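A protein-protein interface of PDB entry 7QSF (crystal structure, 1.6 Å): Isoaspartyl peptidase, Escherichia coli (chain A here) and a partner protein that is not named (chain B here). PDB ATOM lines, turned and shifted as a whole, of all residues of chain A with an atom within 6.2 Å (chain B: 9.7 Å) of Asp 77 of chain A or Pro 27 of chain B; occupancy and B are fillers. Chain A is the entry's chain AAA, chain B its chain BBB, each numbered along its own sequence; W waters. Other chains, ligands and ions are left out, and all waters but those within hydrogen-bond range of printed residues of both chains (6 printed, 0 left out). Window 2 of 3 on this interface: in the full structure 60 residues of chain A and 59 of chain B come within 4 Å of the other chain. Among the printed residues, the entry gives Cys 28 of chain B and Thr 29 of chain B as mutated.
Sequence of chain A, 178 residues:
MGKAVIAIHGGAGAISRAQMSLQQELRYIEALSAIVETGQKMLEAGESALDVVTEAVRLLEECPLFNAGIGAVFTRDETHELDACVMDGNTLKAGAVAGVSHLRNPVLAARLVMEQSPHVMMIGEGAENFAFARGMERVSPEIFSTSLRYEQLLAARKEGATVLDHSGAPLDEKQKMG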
ATOM      1  N   PHE A  74     -15.511   4.816   7.892  1.00  0.00           N
ATOM      2  CA  PHE A  74     -14.236   5.544   8.036  1.00  0.00           C
ATOM      3  C   PHE A  74     -14.431   7.012   7.628  1.00  0.00           C
ATOM      4  O   PHE A  74     -15.135   7.296   6.640  1.00  0.00           O
ATOM      5  CB  PHE A  74     -13.160   4.903   7.164  1.00  0.00           C
ATOM      6  CG  PHE A  74     -12.638   3.571   7.646  1.00  0.00           C
ATOM      7  CD1 PHE A  74     -13.249   2.378   7.307  1.00  0.00           C
ATOM      8  CD2 PHE A  74     -11.464   3.532   8.387  1.00  0.00           C
ATOM      9  CE1 PHE A  74     -12.720   1.165   7.725  1.00  0.00           C
ATOM     10  CE2 PHE A  74     -10.929   2.321   8.782  1.00  0.00           C
ATOM     11  CZ  PHE A  74     -11.548   1.142   8.445  1.00  0.00           C
ATOM     12  N   THR A  75     -13.751   7.905   8.335  1.00  0.00           N
ATOM     13  CA  THR A  75     -13.658   9.353   8.028  1.00  0.00           C
ATOM     14  C   THR A  75     -12.639   9.561   6.892  1.00  0.00           C
ATOM     15  O   THR A  75     -11.945   8.584   6.447  1.00  0.00           O
ATOM     16  CB  THR A  75     -13.207  10.178   9.248  1.00  0.00           C
ATOM     17  OG1 THR A  75     -11.839   9.823   9.513  1.00  0.00           O
ATOM     18  CG2 THR A  75     -14.010   9.943  10.515  1.00  0.00           C
ATOM     19  N   ARG A  76     -12.504  10.819   6.491  1.00  0.00           N
ATOM     20  CA  ARG A  76     -11.470  11.254   5.515  1.00  0.00           C
ATOM     21  C   ARG A  76     -10.062  10.860   5.966  1.00  0.00           C
ATOM     22  O   ARG A  76      -9.207  10.567   5.074  1.00  0.00           O
ATOM     23  CB  ARG A  76     -11.624  12.768   5.391  1.00  0.00           C
ATOM     24  CG  ARG A  76     -10.687  13.430   4.412  1.00  0.00           C
ATOM     25  CD  ARG A  76     -11.023  14.910   4.430  1.00  0.00           C
ATOM     26  NE  ARG A  76      -9.871  15.601   3.899  1.00  0.00           N
ATOM     27  CZ  ARG A  76      -9.605  15.757   2.611  1.00  0.00           C
ATOM     28  NH1 ARG A  76      -8.485  16.353   2.248  1.00  0.00           N
ATOM     29  NH2 ARG A  76     -10.436  15.285   1.693  1.00  0.00           N
ATOM     30  N   ASP A  77      -9.792  10.855   7.275  1.00  0.00           N
ATOM     31  CA  ASP A  77      -8.417  10.654   7.818  1.00  0.00           C
ATOM     32  C   ASP A  77      -8.210   9.168   8.177  1.00  0.00           C
ATOM     33  O   ASP A  77      -7.249   8.846   8.873  1.00  0.00           O
ATOM     34  CB  ASP A  77      -8.209  11.573   9.027  1.00  0.00           C
ATOM     35  CG  ASP A  77      -8.142  13.064   8.707  1.00  0.00           C
ATOM     36  OD1 ASP A  77      -7.979  13.417   7.544  1.00  0.00           O
ATOM     37  OD2 ASP A  77      -8.161  13.858   9.644  1.00  0.00           O
ATOM     38  N   GLU A  78      -9.117   8.295   7.737  1.00  0.00           N
ATOM     39  CA  GLU A  78      -9.110   6.816   7.916  1.00  0.00           C
ATOM     40  C   GLU A  78      -9.269   6.501   9.409  1.00  0.00           C
ATOM     41  O   GLU A  78      -8.703   5.519   9.864  1.00  0.00           O
ATOM     42  CB  GLU A  78      -7.884   6.162   7.274  1.00  0.00           C
ATOM     43  CG  GLU A  78      -7.700   6.534   5.812  1.00  0.00           C
ATOM     44  CD  GLU A  78      -6.513   5.858   5.142  1.00  0.00           C
ATOM     45  OE1 GLU A  78      -5.953   4.901   5.735  1.00  0.00           O
ATOM     46  OE2 GLU A  78      -6.143   6.303   4.048  1.00  0.00           O
ATOM     47  N   THR A  79     -10.032   7.334  10.114  1.00  0.00           N
ATOM     48  CA  THR A  79     -10.328   7.204  11.572  1.00  0.00           C
ATOM     49  C   THR A  79     -11.810   6.828  11.706  1.00  0.00           C
ATOM     50  O   THR A  79     -12.500   6.648  10.650  1.00  0.00           O
ATOM     51  CB  THR A  79      -9.964   8.504  12.329  1.00  0.00           C
ATOM     52  OG1 THR A  79     -10.762   9.586  11.843  1.00  0.00           O
ATOM     53  CG2 THR A  79      -8.506   8.902  12.213  1.00  0.00           C
ATOM     54  N   GLU A  81     -15.309   8.320  14.077  1.00  0.00           N
ATOM     55  CA  GLU A  81     -15.881   9.321  15.022  1.00  0.00           C
ATOM     56  C   GLU A  81     -17.365   9.028  15.181  1.00  0.00           C
ATOM     57  O   GLU A  81     -18.053   9.099  14.156  1.00  0.00           O
ATOM     58  CB  GLU A  81     -15.697  10.777  14.584  1.00  0.00           C
ATOM     59  CG  GLU A  81     -14.243  11.185  14.545  1.00  0.00           C
ATOM     60  CD  GLU A  81     -13.931  12.666  14.394  1.00  0.00           C
ATOM     61  OE1 GLU A  81     -14.863  13.488  14.320  1.00  0.00           O
ATOM     62  OE2 GLU A  81     -12.728  12.974  14.352  1.00  0.00           O
ATOM     63  N   LEU A 153     -14.609   3.066   1.515  1.00  0.00           N
ATOM     64  CA  LEU A 153     -13.802   4.314   1.569  1.00  0.00           C
ATOM     65  C   LEU A 153     -12.965   4.412   0.275  1.00  0.00           C
ATOM     66  O   LEU A 153     -13.024   5.478  -0.412  1.00  0.00           O
ATOM     67  CB  LEU A 153     -12.923   4.360   2.828  1.00  0.00           C
ATOM     68  CG  LEU A 153     -12.058   5.623   2.988  1.00  0.00           C
ATOM     69  CD1 LEU A 153     -12.904   6.874   3.182  1.00  0.00           C
ATOM     70  CD2 LEU A 153     -11.072   5.503   4.130  1.00  0.00           C
ATOM     71  N   GLY B  20     -21.816   5.930  13.056  1.00  0.00           N
ATOM     72  CA  GLY B  20     -20.502   6.467  12.629  1.00  0.00           C
ATOM     73  C   GLY B  20     -20.531   7.517  11.524  1.00  0.00           C
ATOM     74  O   GLY B  20     -19.440   7.988  11.101  1.00  0.00           O
ATOM     75  N   MET B  22     -21.113   9.297   7.779  1.00  0.00           N
ATOM     76  CA  MET B  22     -20.991   8.970   6.336  1.00  0.00           C
ATOM     77  C   MET B  22     -19.525   8.702   5.973  1.00  0.00           C
ATOM     78  O   MET B  22     -18.590   9.402   6.455  1.00  0.00           O
ATOM     79  CB  MET B  22     -21.548  10.106   5.483  1.00  0.00           C
ATOM     80  CG  MET B  22     -23.031  10.396   5.771  1.00  0.00           C
ATOM     81  SD  MET B  22     -24.179   9.031   5.359  1.00  0.00           S
ATOM     82  CE  MET B  22     -25.105   8.869   6.887  1.00  0.00           C
ATOM     83  N   THR B  23     -19.325   7.695   5.131  1.00  0.00           N
ATOM     84  CA  THR B  23     -17.998   7.353   4.563  1.00  0.00           C
ATOM     85  C   THR B  23     -17.328   8.639   4.026  1.00  0.00           C
ATOM     86  O   THR B  23     -17.938   9.412   3.258  1.00  0.00           O
ATOM     87  CB  THR B  23     -18.119   6.223   3.534  1.00  0.00           C
ATOM     88  OG1 THR B  23     -18.479   5.003   4.175  1.00  0.00           O
ATOM     89  CG2 THR B  23     -16.821   5.960   2.801  1.00  0.00           C
ATOM     90  N   ASN B  24     -16.071   8.829   4.385  1.00  0.00           N
ATOM     91  CA  ASN B  24     -15.181   9.927   3.911  1.00  0.00           C
ATOM     92  C   ASN B  24     -15.562  11.261   4.556  1.00  0.00           C
ATOM     93  O   ASN B  24     -15.076  12.288   4.075  1.00  0.00           O
ATOM     94  CB  ASN B  24     -15.103   9.988   2.378  1.00  0.00           C
ATOM     95  CG  ASN B  24     -13.741  10.413   1.850  1.00  0.00           C
ATOM     96  OD1 ASN B  24     -12.714  10.318   2.527  1.00  0.00           O
ATOM     97  ND2 ASN B  24     -13.709  10.817   0.590  1.00  0.00           N
ATOM     98  N   LYS B  25     -16.319  11.264   5.668  1.00  0.00           N
ATOM     99  CA  LYS B  25     -16.692  12.543   6.346  1.00  0.00           C
ATOM    100  C   LYS B  25     -15.445  13.260   6.879  1.00  0.00           C
ATOM    101  O   LYS B  25     -14.448  12.602   7.301  1.00  0.00           O
ATOM    102  CB  LYS B  25     -17.695  12.380   7.500  1.00  0.00           C
ATOM    103  CG  LYS B  25     -17.265  11.578   8.722  1.00  0.00           C
ATOM    104  CD  LYS B  25     -18.308  11.551   9.872  1.00  0.00           C
ATOM    105  CE  LYS B  25     -17.831  10.896  11.162  1.00  0.00           C
ATOM    106  NZ  LYS B  25     -18.834  10.987  12.255  1.00  0.00           N
ATOM    107  N   LEU B  26     -15.475  14.578   6.842  1.00  0.00           N
ATOM    108  CA  LEU B  26     -14.516  15.435   7.568  1.00  0.00           C
ATOM    109  C   LEU B  26     -14.716  15.201   9.070  1.00  0.00           C
ATOM    110  O   LEU B  26     -15.860  15.148   9.557  1.00  0.00           O
ATOM    111  CB  LEU B  26     -14.787  16.890   7.187  1.00  0.00           C
ATOM    112  CG  LEU B  26     -13.760  17.914   7.649  1.00  0.00           C
ATOM    113  CD1 LEU B  26     -12.455  17.824   6.858  1.00  0.00           C
ATOM    114  CD2 LEU B  26     -14.334  19.325   7.585  1.00  0.00           C
ATOM    115  N   PRO B  27     -13.622  15.061   9.856  1.00  0.00           N
ATOM    116  CA  PRO B  27     -13.765  14.956  11.305  1.00  0.00           C
ATOM    117  C   PRO B  27     -14.383  16.243  11.893  1.00  0.00           C
ATOM    118  O   PRO B  27     -14.293  17.286  11.258  1.00  0.00           O
ATOM    119  CB  PRO B  27     -12.330  14.799  11.821  1.00  0.00           C
ATOM    120  CG  PRO B  27     -11.475  14.502  10.616  1.00  0.00           C
ATOM    121  CD  PRO B  27     -12.237  14.949   9.392  1.00  0.00           C
ATOM    122  N   CYS B  28     -14.885  16.129  13.113  1.00  0.00           N
ATOM    123  CA  CYS B  28     -15.462  17.223  13.941  1.00  0.00           C
ATOM    124  C   CYS B  28     -16.756  17.767  13.313  1.00  0.00           C
ATOM    125  O   CYS B  28     -17.088  18.956  13.544  1.00  0.00           O
ATOM    126  CB  CYS B  28     -14.460  18.339  14.199  1.00  0.00           C
ATOM    127  SG  CYS B  28     -13.013  17.864  15.185  1.00  0.00           S
ATOM    128  N   THR B  29     -17.464  16.936  12.549  1.00  0.00           N
ATOM    129  CA  THR B  29     -18.795  17.261  11.971  1.00  0.00           C
ATOM    130  C   THR B  29     -19.853  16.471  12.751  1.00  0.00           C
ATOM    131  O   THR B  29     -19.512  15.342  13.190  1.00  0.00           O
ATOM    132  CB  THR B  29     -18.781  17.010  10.463  1.00  0.00           C
ATOM    133  OG1 THR B  29     -18.473  15.637  10.245  1.00  0.00           O
ATOM    134  CG2 THR B  29     -17.745  17.865   9.761  1.00  0.00           C
ATOM    135  N   VAL B  30     -21.075  17.019  12.908  1.00  0.00           N
ATOM    136  CA  VAL B  30     -22.155  16.409  13.749  1.00  0.00           C
ATOM    137  C   VAL B  30     -23.446  16.420  12.924  1.00  0.00           C
ATOM    138  O   VAL B  30     -23.838  17.498  12.441  1.00  0.00           O
ATOM    139  CB  VAL B  30     -22.354  17.121  15.108  1.00  0.00           C
ATOM    140  CG1 VAL B  30     -23.426  16.439  15.948  1.00  0.00           C
ATOM    141  CG2 VAL B  30     -21.062  17.218  15.930  1.00  0.00           C
HETATM  142  O   HOH W   1     -12.218  14.545  16.471  1.00  0.00           O
HETATM  143  O   HOH W   2     -17.185  13.582  12.930  1.00  0.00           O
HETATM  144  O   HOH W   3     -10.002   9.777   2.489  1.00  0.00           O
HETATM  145  O   HOH W   4     -16.529  14.836  15.741  1.00  0.00           O
HETATM  146  O   HOH W   5     -16.742   7.191  11.775  1.00  0.00           O
HETATM  147  O   HOH W   6     -16.232   3.584   5.269  1.00  0.00           O
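The backbone carbonyl oxygen (O) of Phe 74 of chain A is in hydrogen-bond range of the backbone NH (N) of Asn 24 of chain B.
N of Arg 76 of chain A is in hydrogen-bond range of O of Lys 25 of chain B.
The backbone carbonyl oxygen (O) of Glu 81 of chain A lies within hydrogen-bond range of the side-chain amino group (NZ) of Lys 25 of chain B, 2.8 Å away.
OE1 of Glu 81 of chain A lies within hydrogen-bond range of N of Cys 28 of chain B, 2.9 Å away.
OG1 of Thr 75 of chain A sits close to N of Asp 77 of chain A (3.2 Å).
The side-chain hydroxyl of Thr 75 of chain A lies within hydrogen-bond range of the side-chain hydroxyl of Thr 79 of chain A.
The backbone carbonyl oxygen (O) of Gly 20 of chain B sits at hydrogen-bond distance from the side-chain amino group (NZ) of Lys 25 of chain B (3.3 Å).
Phe 74 of chain A touches Thr 23 of chain B.
CA of Asn 24 of chain B touches C of Thr 75 of chain A, 3.9 Å away.
Thr 75 of chain A touches Lys 25 of chain B.
CA of Arg 76 of chain A touches OD1 of Asn 24 of chain B, at 3.4 Å.
Asp 77 of chain A touches Pro 27 of chain B (OD2 to CG, 3.5 Å).
Gly 20 of chain B touches Glu 81 of chain A.
CB of Pro 27 of chain B touches OE2 of Glu 81 of chain A, at 3.1 Å.
Leu 153 of chain A touches Thr 23 of chain B (CA to CG2, 3.7 Å).
Leu 153 of chain A touches Asn 24 of chain B.
Of chain B, only Pro 27 comes within 4 Å of Asp 77 of chain A.
Printed residues of chain A within 4 Å of Pro 27 of chain B: Asp 77 (3.5 Å) and Glu 81 (3.1 Å).
No residue of chain B comes within 4 Å of Thr 79 of chain A.
Of the printed residues of chain A, Lys 25 of chain B touches Thr 75, Arg 76 and Glu 81.
Of the printed residues of chain B, Glu 81 of chain A touches Gly 20, Lys 25, Pro 27 and Cys 28.
The nearest residue of chain A that does not touch Pro 27 of chain B is Arg 76 of chain A (4.6 Å).
Printed residues of chain B that touch a printed residue of chain A: Gly 20, Thr 23, Asn 24, Lys 25, Pro 27 and Cys 28.
Hydrophobic or aromatic side chains of chain B that line the printed part of chain A: Pro 27.
Printed residues of chain A that touch a printed residue of chain B: Phe 74, Thr 75, Arg 76, Asp 77, Glu 81 and Leu 153.
Hydrophobic or aromatic side chains of chain A within 4 Å of the printed part of chain B: Leu 153.
Among the printed residues, 13 pairs touch across the chains.
Water W4 bridges OE1 of Glu 81 of chain A and N of Cys 28 of chain B.
Water W1 lies within hydrogen-bond range of the side-chain carboxylate of Glu 81 of chain A and the side-chain sulfur of Cys 28 of chain B.
Water W2 lies within hydrogen-bond range of OE1 of Glu 81 of chain A (2.7 Å), O of Thr 29 of chain B (2.9 Å), NZ of Lys 25 of chain B (3.1 Å) and N of Cys 28 of chain B (3.4 Å).
Water W3 lies within hydrogen-bond range of OD1 of Asn 24 of chain B and O of Arg 76 of chain A.
Water W6 bridges the side-chain hydroxyl of Thr 23 of chain B (2.9 Å) and the backbone NH of Phe 74 of chain A (3.0 Å).
Water W5 lies within hydrogen-bond range of O of Gly 20 of chain B (2.9 Å) and N of Glu 81 of chain A (2.9 Å).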
